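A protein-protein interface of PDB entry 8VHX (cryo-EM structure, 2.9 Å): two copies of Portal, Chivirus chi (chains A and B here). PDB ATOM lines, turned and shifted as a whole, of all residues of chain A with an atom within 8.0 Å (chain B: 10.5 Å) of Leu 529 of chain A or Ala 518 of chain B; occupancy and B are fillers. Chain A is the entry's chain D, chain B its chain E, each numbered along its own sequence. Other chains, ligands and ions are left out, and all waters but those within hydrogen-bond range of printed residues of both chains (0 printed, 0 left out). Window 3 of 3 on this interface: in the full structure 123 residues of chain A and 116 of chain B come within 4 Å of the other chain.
Of the printed residues of chain B, Ile 524 of chain A touches Phe 514 (3.5 Å).
Leu 527 of chain A touches just one residue of chain B: Phe 514.
Leu 529 of chain A touches just these residues of chain B: Phe 514 (3.7 Å), Arg 517 (3.9 Å) and Ala 518 (3.8 Å).
No residue of chain B comes within 4 Å of Asp 530 of chain A.
Printed residues of chain A within 4 Å of Phe 510 of chain B: Glu 520 and Ile 523.
Val 513 of chain B touches none of the printed residues of chain A.
Of the printed residues of chain A, Arg 517 of chain B touches Leu 529.
Ala 518 of chain B touches just one residue of chain A: Leu 529 (3.8 Å).
Arg 519 of chain B touches none of the printed residues of chain A.
The nearest residue of chain A that does not touch Ala 518 of chain B is Leu 527 of chain A (4.3 Å).
The nearest printed residue of chain A that does not touch Arg 511 of chain B is Leu 527 of chain A (5.4 Å).
The backbone NH (N) of Leu 529 of chain A lies within hydrogen-bond range of the backbone carbonyl oxygen (O) of Ile 524 of chain A.
OE2 of Glu 521 of chain B is in salt-bridge range of NH1 of Arg 517 of chain B (3.2 Å).
The backbone NH (N) of Tyr 499 of chain B sits at hydrogen-bond distance from the side-chain carboxylate (OE1) of Glu 520 of chain A, 2.9 Å away.
Printed residues of chain A that touch a printed residue of chain B: Glu 520, Glu 521, Ile 523, Ile 524, Leu 527, Leu 529 and Phe 531.
Among the printed residues, 12 pairs touch across the chains.
Among the printed residues, no Asp or Glu carboxylate lies within 4 Å of a Lys or Arg side-chain nitrogen of the other chain.
Phe 510 of chain B touches Glu 520 of chain A.
Tyr 499 of chain B touches Glu 521 of chain A (CE2 to OE2, 3.9 Å).
CD1 of Ile 523 of chain A touches CE2 of Phe 510 of chain B, 3.6 Å away.
CD1 of Ile 523 of chain A touches NE of Arg 511 of chain B (3.96 Å).
Phe 514 of chain B touches Ile 523 of chain A.
Ile 524 of chain A touches Phe 514 of chain B (CG1 to CE2, 3.5 Å).
Phe 514 of chain B touches Leu 527 of chain A (CB to CD1, 3.5 Å).
Phe 514 of chain B touches Leu 529 of chain A.
Leu 529 of chain A touches Arg 517 of chain B (CD2 to C, 3.9 Å).
CD2 of Leu 529 of chain A touches N of Ala 518 of chain B, at 3.8 Å.
Positions printed for both chains: 520, 521, 523, 524, 525 and 526.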
ATOM      1  N   GLU A 520       9.583 -21.606  -7.151  1.00  0.00           N
ATOM      2  CA  GLU A 520       8.634 -21.649  -8.259  1.00  0.00           C
ATOM      3  C   GLU A 520       8.497 -20.291  -8.936  1.00  0.00           C
ATOM      4  O   GLU A 520       8.411 -20.211 -10.164  1.00  0.00           O
ATOM      5  CB  GLU A 520       7.279 -22.145  -7.763  1.00  0.00           C
ATOM      6  CG  GLU A 520       7.249 -23.627  -7.459  1.00  0.00           C
ATOM      7  CD  GLU A 520       6.115 -24.022  -6.536  1.00  0.00           C
ATOM      8  OE1 GLU A 520       5.301 -23.152  -6.176  1.00  0.00           O
ATOM      9  OE2 GLU A 520       6.037 -25.214  -6.172  1.00  0.00           O
ATOM     10  N   GLU A 521       8.452 -19.212  -8.154  1.00  0.00           N
ATOM     11  CA  GLU A 521       8.382 -17.879  -8.743  1.00  0.00           C
ATOM     12  C   GLU A 521       9.655 -17.556  -9.512  1.00  0.00           C
ATOM     13  O   GLU A 521       9.605 -16.925 -10.574  1.00  0.00           O
ATOM     14  CB  GLU A 521       8.137 -16.825  -7.664  1.00  0.00           C
ATOM     15  CG  GLU A 521       6.821 -16.952  -6.909  1.00  0.00           C
ATOM     16  CD  GLU A 521       5.616 -16.966  -7.814  1.00  0.00           C
ATOM     17  OE1 GLU A 521       5.685 -16.373  -8.908  1.00  0.00           O
ATOM     18  OE2 GLU A 521       4.591 -17.565  -7.422  1.00  0.00           O
ATOM     19  N   ILE A 523      11.549 -19.778 -11.022  1.00  0.00           N
ATOM     20  CA  ILE A 523      11.484 -20.578 -12.241  1.00  0.00           C
ATOM     21  C   ILE A 523      10.531 -19.949 -13.248  1.00  0.00           C
ATOM     22  O   ILE A 523      10.859 -19.818 -14.432  1.00  0.00           O
ATOM     23  CB  ILE A 523      11.074 -22.019 -11.900  1.00  0.00           C
ATOM     24  CG1 ILE A 523      12.239 -22.756 -11.237  1.00  0.00           C
ATOM     25  CG2 ILE A 523      10.603 -22.729 -13.135  1.00  0.00           C
ATOM     26  CD1 ILE A 523      11.838 -24.048 -10.563  1.00  0.00           C
ATOM     27  N   ILE A 524       9.338 -19.560 -12.798  1.00  0.00           N
ATOM     28  CA  ILE A 524       8.389 -18.888 -13.679  1.00  0.00           C
ATOM     29  C   ILE A 524       9.045 -17.677 -14.319  1.00  0.00           C
ATOM     30  O   ILE A 524       9.027 -17.505 -15.543  1.00  0.00           O
ATOM     31  CB  ILE A 524       7.135 -18.476 -12.894  1.00  0.00           C
ATOM     32  CG1 ILE A 524       6.246 -19.683 -12.612  1.00  0.00           C
ATOM     33  CG2 ILE A 524       6.373 -17.427 -13.661  1.00  0.00           C
ATOM     34  CD1 ILE A 524       5.277 -19.457 -11.451  1.00  0.00           C
ATOM     35  N   LYS A 525       9.645 -16.825 -13.491  1.00  0.00           N
ATOM     36  CA  LYS A 525      10.278 -15.617 -14.000  1.00  0.00           C
ATOM     37  C   LYS A 525      11.359 -15.951 -15.016  1.00  0.00           C
ATOM     38  O   LYS A 525      11.507 -15.256 -16.028  1.00  0.00           O
ATOM     39  CB  LYS A 525      10.853 -14.817 -12.836  1.00  0.00           C
ATOM     40  CG  LYS A 525      11.862 -13.778 -13.233  1.00  0.00           C
ATOM     41  CD  LYS A 525      13.256 -14.308 -13.008  1.00  0.00           C
ATOM     42  CE  LYS A 525      14.288 -13.507 -13.764  1.00  0.00           C
ATOM     43  NZ  LYS A 525      15.643 -14.106 -13.634  1.00  0.00           N
ATOM     44  N   ASP A 526      12.126 -17.010 -14.765  1.00  0.00           N
ATOM     45  CA  ASP A 526      13.191 -17.379 -15.689  1.00  0.00           C
ATOM     46  C   ASP A 526      12.638 -17.944 -16.988  1.00  0.00           C
ATOM     47  O   ASP A 526      13.221 -17.721 -18.054  1.00  0.00           O
ATOM     48  CB  ASP A 526      14.123 -18.386 -15.020  1.00  0.00           C
ATOM     49  CG  ASP A 526      15.121 -17.727 -14.092  1.00  0.00           C
ATOM     50  OD1 ASP A 526      15.368 -16.514 -14.251  1.00  0.00           O
ATOM     51  OD2 ASP A 526      15.662 -18.418 -13.205  1.00  0.00           O
ATOM     52  N   LEU A 527      11.527 -18.672 -16.922  1.00  0.00           N
ATOM     53  CA  LEU A 527      10.898 -19.207 -18.121  1.00  0.00           C
ATOM     54  C   LEU A 527      10.042 -18.183 -18.849  1.00  0.00           C
ATOM     55  O   LEU A 527       9.661 -18.424 -19.997  1.00  0.00           O
ATOM     56  CB  LEU A 527      10.034 -20.416 -17.767  1.00  0.00           C
ATOM     57  CG  LEU A 527      10.768 -21.657 -17.268  1.00  0.00           C
ATOM     58  CD1 LEU A 527       9.785 -22.732 -16.875  1.00  0.00           C
ATOM     59  CD2 LEU A 527      11.710 -22.183 -18.318  1.00  0.00           C
ATOM     60  N   GLY A 528       9.718 -17.065 -18.209  1.00  0.00           N
ATOM     61  CA  GLY A 528       8.894 -16.059 -18.844  1.00  0.00           C
ATOM     62  C   GLY A 528       7.425 -16.405 -18.897  1.00  0.00           C
ATOM     63  O   GLY A 528       6.722 -15.956 -19.808  1.00  0.00           O
ATOM     64  N   LEU A 529       6.940 -17.194 -17.945  1.00  0.00           N
ATOM     65  CA  LEU A 529       5.547 -17.602 -17.921  1.00  0.00           C
ATOM     66  C   LEU A 529       4.691 -16.567 -17.200  1.00  0.00           C
ATOM     67  O   LEU A 529       5.183 -15.717 -16.455  1.00  0.00           O
ATOM     68  CB  LEU A 529       5.398 -18.960 -17.239  1.00  0.00           C
ATOM     69  CG  LEU A 529       6.005 -20.168 -17.935  1.00  0.00           C
ATOM     70  CD1 LEU A 529       5.789 -21.390 -17.075  1.00  0.00           C
ATOM     71  CD2 LEU A 529       5.385 -20.363 -19.305  1.00  0.00           C
ATOM     72  N   ASP A 530       3.380 -16.644 -17.449  1.00  0.00           N
ATOM     73  CA  ASP A 530       2.397 -15.759 -16.834  1.00  0.00           C
ATOM     74  C   ASP A 530       1.164 -16.587 -16.466  1.00  0.00           C
ATOM     75  O   ASP A 530       0.261 -16.794 -17.279  1.00  0.00           O
ATOM     76  CB  ASP A 530       2.040 -14.608 -17.766  1.00  0.00           C
ATOM     77  CG  ASP A 530       0.950 -13.722 -17.205  1.00  0.00           C
ATOM     78  OD1 ASP A 530       0.693 -13.781 -15.984  1.00  0.00           O
ATOM     79  OD2 ASP A 530       0.330 -12.988 -17.996  1.00  0.00           O
ATOM     80  N   PHE A 531       1.127 -17.062 -15.228  1.00  0.00           N
ATOM     81  CA  PHE A 531      -0.061 -17.711 -14.695  1.00  0.00           C
ATOM     82  C   PHE A 531      -0.994 -16.676 -14.081  1.00  0.00           C
ATOM     83  O   PHE A 531      -0.544 -15.650 -13.571  1.00  0.00           O
ATOM     84  CB  PHE A 531       0.322 -18.756 -13.655  1.00  0.00           C
ATOM     85  CG  PHE A 531       0.934 -19.991 -14.231  1.00  0.00           C
ATOM     86  CD1 PHE A 531       0.168 -21.119 -14.483  1.00  0.00           C
ATOM     87  CD2 PHE A 531       2.275 -20.019 -14.544  1.00  0.00           C
ATOM     88  CE1 PHE A 531       0.739 -22.248 -15.010  1.00  0.00           C
ATOM     89  CE2 PHE A 531       2.847 -21.142 -15.076  1.00  0.00           C
ATOM     90  CZ  PHE A 531       2.083 -22.257 -15.312  1.00  0.00           C
ATOM     91  N   TYR B 499       2.850 -24.668  -6.127  1.00  0.00           N
ATOM     92  CA  TYR B 499       2.481 -25.330  -7.369  1.00  0.00           C
ATOM     93  C   TYR B 499       2.836 -26.808  -7.315  1.00  0.00           C
ATOM     94  O   TYR B 499       2.060 -27.661  -7.755  1.00  0.00           O
ATOM     95  CB  TYR B 499       3.181 -24.656  -8.539  1.00  0.00           C
ATOM     96  CG  TYR B 499       2.707 -23.254  -8.826  1.00  0.00           C
ATOM     97  CD1 TYR B 499       1.632 -23.017  -9.667  1.00  0.00           C
ATOM     98  CD2 TYR B 499       3.348 -22.164  -8.271  1.00  0.00           C
ATOM     99  CE1 TYR B 499       1.212 -21.743  -9.933  1.00  0.00           C
ATOM    100  CE2 TYR B 499       2.930 -20.886  -8.534  1.00  0.00           C
ATOM    101  CZ  TYR B 499       1.861 -20.680  -9.367  1.00  0.00           C
ATOM    102  OH  TYR B 499       1.435 -19.403  -9.634  1.00  0.00           O
ATOM    103  N   ILE B 503       0.005 -29.476  -8.232  1.00  0.00           N
ATOM    104  CA  ILE B 503       0.164 -30.216  -9.471  1.00  0.00           C
ATOM    105  C   ILE B 503       0.387 -31.689  -9.180  1.00  0.00           C
ATOM    106  O   ILE B 503      -0.029 -32.554  -9.959  1.00  0.00           O
ATOM    107  CB  ILE B 503       1.308 -29.607 -10.292  1.00  0.00           C
ATOM    108  CG1 ILE B 503       0.989 -28.154 -10.624  1.00  0.00           C
ATOM    109  CG2 ILE B 503       1.502 -30.361 -11.561  1.00  0.00           C
ATOM    110  CD1 ILE B 503       2.116 -27.419 -11.261  1.00  0.00           C
ATOM    111  N   PHE B 510       5.821 -30.054 -10.928  1.00  0.00           N
ATOM    112  CA  PHE B 510       5.604 -28.722 -11.474  1.00  0.00           C
ATOM    113  C   PHE B 510       6.649 -28.326 -12.508  1.00  0.00           C
ATOM    114  O   PHE B 510       6.362 -27.504 -13.385  1.00  0.00           O
ATOM    115  CB  PHE B 510       5.572 -27.704 -10.342  1.00  0.00           C
ATOM    116  CG  PHE B 510       6.924 -27.322  -9.832  1.00  0.00           C
ATOM    117  CD1 PHE B 510       7.592 -28.130  -8.933  1.00  0.00           C
ATOM    118  CD2 PHE B 510       7.533 -26.156 -10.251  1.00  0.00           C
ATOM    119  CE1 PHE B 510       8.830 -27.781  -8.464  1.00  0.00           C
ATOM    120  CE2 PHE B 510       8.769 -25.809  -9.784  1.00  0.00           C
ATOM    121  CZ  PHE B 510       9.419 -26.623  -8.890  1.00  0.00           C
ATOM    122  N   ARG B 511       7.857 -28.881 -12.441  1.00  0.00           N
ATOM    123  CA  ARG B 511       8.925 -28.323 -13.261  1.00  0.00           C
ATOM    124  C   ARG B 511       8.805 -28.753 -14.716  1.00  0.00           C
ATOM    125  O   ARG B 511       8.979 -27.933 -15.625  1.00  0.00           O
ATOM    126  CB  ARG B 511      10.288 -28.711 -12.703  1.00  0.00           C
ATOM    127  CG  ARG B 511      11.409 -27.959 -13.386  1.00  0.00           C
ATOM    128  CD  ARG B 511      12.776 -28.326 -12.861  1.00  0.00           C
ATOM    129  NE  ARG B 511      13.063 -27.669 -11.590  1.00  0.00           N
ATOM    130  CZ  ARG B 511      13.032 -28.265 -10.402  1.00  0.00           C
ATOM    131  NH1 ARG B 511      13.315 -27.565  -9.315  1.00  0.00           N
ATOM    132  NH2 ARG B 511      12.718 -29.550 -10.290  1.00  0.00           N
ATOM    133  N   GLU B 512       8.508 -30.028 -14.963  1.00  0.00           N
ATOM    134  CA  GLU B 512       8.261 -30.445 -16.336  1.00  0.00           C
ATOM    135  C   GLU B 512       7.027 -29.750 -16.889  1.00  0.00           C
ATOM    136  O   GLU B 512       6.974 -29.434 -18.080  1.00  0.00           O
ATOM    137  CB  GLU B 512       8.103 -31.964 -16.415  1.00  0.00           C
ATOM    138  CG  GLU B 512       6.701 -32.466 -16.137  1.00  0.00           C
ATOM    139  CD  GLU B 512       6.606 -33.978 -16.202  1.00  0.00           C
ATOM    140  OE1 GLU B 512       7.599 -34.617 -16.600  1.00  0.00           O
ATOM    141  OE2 GLU B 512       5.533 -34.524 -15.864  1.00  0.00           O
ATOM    142  N   VAL B 513       6.037 -29.494 -16.034  1.00  0.00           N
ATOM    143  CA  VAL B 513       4.848 -28.764 -16.456  1.00  0.00           C
ATOM    144  C   VAL B 513       5.220 -27.360 -16.906  1.00  0.00           C
ATOM    145  O   VAL B 513       4.724 -26.865 -17.925  1.00  0.00           O
ATOM    146  CB  VAL B 513       3.822 -28.738 -15.312  1.00  0.00           C
ATOM    147  CG1 VAL B 513       2.716 -27.763 -15.605  1.00  0.00           C
ATOM    148  CG2 VAL B 513       3.264 -30.121 -15.086  1.00  0.00           C
ATOM    149  N   PHE B 514       6.101 -26.697 -16.163  1.00  0.00           N
ATOM    150  CA  PHE B 514       6.493 -25.345 -16.535  1.00  0.00           C
ATOM    151  C   PHE B 514       7.342 -25.347 -17.797  1.00  0.00           C
ATOM    152  O   PHE B 514       7.228 -24.442 -18.629  1.00  0.00           O
ATOM    153  CB  PHE B 514       7.238 -24.685 -15.382  1.00  0.00           C
ATOM    154  CG  PHE B 514       6.359 -24.311 -14.226  1.00  0.00           C
ATOM    155  CD1 PHE B 514       5.034 -24.708 -14.178  1.00  0.00           C
ATOM    156  CD2 PHE B 514       6.853 -23.543 -13.194  1.00  0.00           C
ATOM    157  CE1 PHE B 514       4.237 -24.354 -13.118  1.00  0.00           C
ATOM    158  CE2 PHE B 514       6.053 -23.192 -12.141  1.00  0.00           C
ATOM    159  CZ  PHE B 514       4.749 -23.596 -12.104  1.00  0.00           C
ATOM    160  N   LYS B 515       8.200 -26.352 -17.960  1.00  0.00           N
ATOM    161  CA  LYS B 515       8.966 -26.464 -19.197  1.00  0.00           C
ATOM    162  C   LYS B 515       8.042 -26.669 -20.390  1.00  0.00           C
ATOM    163  O   LYS B 515       8.220 -26.051 -21.450  1.00  0.00           O
ATOM    164  CB  LYS B 515       9.957 -27.616 -19.084  1.00  0.00           C
ATOM    165  CG  LYS B 515      11.084 -27.366 -18.099  1.00  0.00           C
ATOM    166  CD  LYS B 515      11.962 -28.592 -17.948  1.00  0.00           C
ATOM    167  CE  LYS B 515      12.994 -28.385 -16.861  1.00  0.00           C
ATOM    168  NZ  LYS B 515      14.018 -27.392 -17.259  1.00  0.00           N
ATOM    169  N   GLN B 516       7.042 -27.535 -20.230  1.00  0.00           N
ATOM    170  CA  GLN B 516       6.081 -27.771 -21.299  1.00  0.00           C
ATOM    171  C   GLN B 516       5.305 -26.506 -21.623  1.00  0.00           C
ATOM    172  O   GLN B 516       5.046 -26.212 -22.793  1.00  0.00           O
ATOM    173  CB  GLN B 516       5.133 -28.895 -20.897  1.00  0.00           C
ATOM    174  CG  GLN B 516       4.183 -29.304 -21.983  1.00  0.00           C
ATOM    175  CD  GLN B 516       4.905 -29.848 -23.191  1.00  0.00           C
ATOM    176  OE1 GLN B 516       6.043 -30.300 -23.093  1.00  0.00           O
ATOM    177  NE2 GLN B 516       4.253 -29.802 -24.338  1.00  0.00           N
ATOM    178  N   ARG B 517       4.902 -25.757 -20.597  1.00  0.00           N
ATOM    179  CA  ARG B 517       4.220 -24.491 -20.836  1.00  0.00           C
ATOM    180  C   ARG B 517       5.133 -23.494 -21.535  1.00  0.00           C
ATOM    181  O   ARG B 517       4.672 -22.694 -22.352  1.00  0.00           O
ATOM    182  CB  ARG B 517       3.697 -23.916 -19.523  1.00  0.00           C
ATOM    183  CG  ARG B 517       2.396 -24.541 -19.039  1.00  0.00           C
ATOM    184  CD  ARG B 517       1.247 -24.209 -19.970  1.00  0.00           C
ATOM    185  NE  ARG B 517       1.066 -22.766 -20.097  1.00  0.00           N
ATOM    186  CZ  ARG B 517       0.102 -22.064 -19.513  1.00  0.00           C
ATOM    187  NH1 ARG B 517       0.055 -20.758 -19.710  1.00  0.00           N
ATOM    188  NH2 ARG B 517      -0.817 -22.648 -18.755  1.00  0.00           N
ATOM    189  N   ALA B 518       6.427 -23.514 -21.224  1.00  0.00           N
ATOM    190  CA  ALA B 518       7.362 -22.667 -21.956  1.00  0.00           C
ATOM    191  C   ALA B 518       7.385 -23.032 -23.433  1.00  0.00           C
ATOM    192  O   ALA B 518       7.346 -22.152 -24.302  1.00  0.00           O
ATOM    193  CB  ALA B 518       8.759 -22.793 -21.362  1.00  0.00           C
ATOM    194  N   ARG B 519       7.433 -24.330 -23.733  1.00  0.00           N
ATOM    195  CA  ARG B 519       7.401 -24.764 -25.127  1.00  0.00           C
ATOM    196  C   ARG B 519       6.102 -24.342 -25.798  1.00  0.00           C
ATOM    197  O   ARG B 519       6.098 -23.882 -26.945  1.00  0.00           O
ATOM    198  CB  ARG B 519       7.564 -26.277 -25.221  1.00  0.00           C
ATOM    199  CG  ARG B 519       8.849 -26.820 -24.634  1.00  0.00           C
ATOM    200  CD  ARG B 519       8.783 -28.326 -24.498  1.00  0.00           C
ATOM    201  NE  ARG B 519       9.749 -28.801 -23.515  1.00  0.00           N
ATOM    202  CZ  ARG B 519       9.558 -29.839 -22.708  1.00  0.00           C
ATOM    203  NH1 ARG B 519      10.503 -30.173 -21.850  1.00  0.00           N
ATOM    204  NH2 ARG B 519       8.434 -30.546 -22.754  1.00  0.00           N
ATOM    205  N   GLU B 520       4.980 -24.522 -25.100  1.00  0.00           N
ATOM    206  CA  GLU B 520       3.683 -24.163 -25.663  1.00  0.00           C
ATOM    207  C   GLU B 520       3.581 -22.665 -25.921  1.00  0.00           C
ATOM    208  O   GLU B 520       3.007 -22.246 -26.928  1.00  0.00           O
ATOM    209  CB  GLU B 520       2.560 -24.626 -24.737  1.00  0.00           C
ATOM    210  CG  GLU B 520       2.370 -26.132 -24.697  1.00  0.00           C
ATOM    211  CD  GLU B 520       1.179 -26.554 -23.855  1.00  0.00           C
ATOM    212  OE1 GLU B 520       0.292 -25.711 -23.612  1.00  0.00           O
ATOM    213  OE2 GLU B 520       1.123 -27.734 -23.449  1.00  0.00           O
ATOM    214  N   GLU B 521       4.109 -21.839 -25.014  1.00  0.00           N
ATOM    215  CA  GLU B 521       4.083 -20.397 -25.234  1.00  0.00           C
ATOM    216  C   GLU B 521       5.013 -19.986 -26.365  1.00  0.00           C
ATOM    217  O   GLU B 521       4.717 -19.037 -27.098  1.00  0.00           O
ATOM    218  CB  GLU B 521       4.460 -19.645 -23.960  1.00  0.00           C
ATOM    219  CG  GLU B 521       3.481 -19.790 -22.814  1.00  0.00           C
ATOM    220  CD  GLU B 521       2.040 -19.615 -23.240  1.00  0.00           C
ATOM    221  OE1 GLU B 521       1.777 -18.759 -24.108  1.00  0.00           O
ATOM    222  OE2 GLU B 521       1.170 -20.332 -22.704  1.00  0.00           O
ATOM    223  N   GLY B 522       6.145 -20.668 -26.515  1.00  0.00           N
ATOM    224  CA  GLY B 522       7.000 -20.393 -27.656  1.00  0.00           C
ATOM    225  C   GLY B 522       6.323 -20.750 -28.960  1.00  0.00           C
ATOM    226  O   GLY B 522       6.419 -20.017 -29.948  1.00  0.00           O
ATOM    227  N   ILE B 523       5.625 -21.884 -28.979  1.00  0.00           N
ATOM    228  CA  ILE B 523       4.880 -22.293 -30.165  1.00  0.00           C
ATOM    229  C   ILE B 523       3.776 -21.288 -30.465  1.00  0.00           C
ATOM    230  O   ILE B 523       3.604 -20.840 -31.604  1.00  0.00           O
ATOM    231  CB  ILE B 523       4.307 -23.706 -29.961  1.00  0.00           C
ATOM    232  CG1 ILE B 523       5.436 -24.730 -29.884  1.00  0.00           C
ATOM    233  CG2 ILE B 523       3.348 -24.060 -31.073  1.00  0.00           C
ATOM    234  CD1 ILE B 523       5.015 -26.030 -29.242  1.00  0.00           C
ATOM    235  N   ILE B 524       3.008 -20.924 -29.439  1.00  0.00           N
ATOM    236  CA  ILE B 524       1.924 -19.967 -29.609  1.00  0.00           C
ATOM    237  C   ILE B 524       2.459 -18.653 -30.152  1.00  0.00           C
ATOM    238  O   ILE B 524       1.884 -18.062 -31.072  1.00  0.00           O
ATOM    239  CB  ILE B 524       1.190 -19.762 -28.272  1.00  0.00           C
ATOM    240  CG1 ILE B 524       0.335 -20.982 -27.930  1.00  0.00           C
ATOM    241  CG2 ILE B 524       0.337 -18.517 -28.326  1.00  0.00           C
ATOM    242  CD1 ILE B 524      -0.108 -21.026 -26.475  1.00  0.00           C
ATOM    243  N   LYS B 525       3.574 -18.182 -29.599  1.00  0.00           N
ATOM    244  CA  LYS B 525       4.093 -16.876 -29.982  1.00  0.00           C
ATOM    245  C   LYS B 525       4.530 -16.846 -31.440  1.00  0.00           C
ATOM    246  O   LYS B 525       4.153 -15.936 -32.186  1.00  0.00           O
ATOM    247  CB  LYS B 525       5.251 -16.495 -29.070  1.00  0.00           C
ATOM    248  CG  LYS B 525       5.860 -15.158 -29.411  1.00  0.00           C
ATOM    249  CD  LYS B 525       6.737 -14.631 -28.300  1.00  0.00           C
ATOM    250  CE  LYS B 525       7.871 -15.582 -27.970  1.00  0.00           C
ATOM    251  NZ  LYS B 525       8.777 -15.049 -26.914  1.00  0.00           N
ATOM    252  N   ASP B 526       5.317 -17.829 -31.870  1.00  0.00           N
ATOM    253  CA  ASP B 526       5.785 -17.832 -33.247  1.00  0.00           C
ATOM    254  C   ASP B 526       4.669 -18.124 -34.238  1.00  0.00           C
ATOM    255  O   ASP B 526       4.794 -17.769 -35.415  1.00  0.00           O
ATOM    256  CB  ASP B 526       6.926 -18.844 -33.400  1.00  0.00           C
ATOM    257  CG  ASP B 526       6.443 -20.286 -33.464  1.00  0.00           C
ATOM    258  OD1 ASP B 526       5.221 -20.532 -33.466  1.00  0.00           O
ATOM    259  OD2 ASP B 526       7.303 -21.186 -33.513  1.00  0.00           O
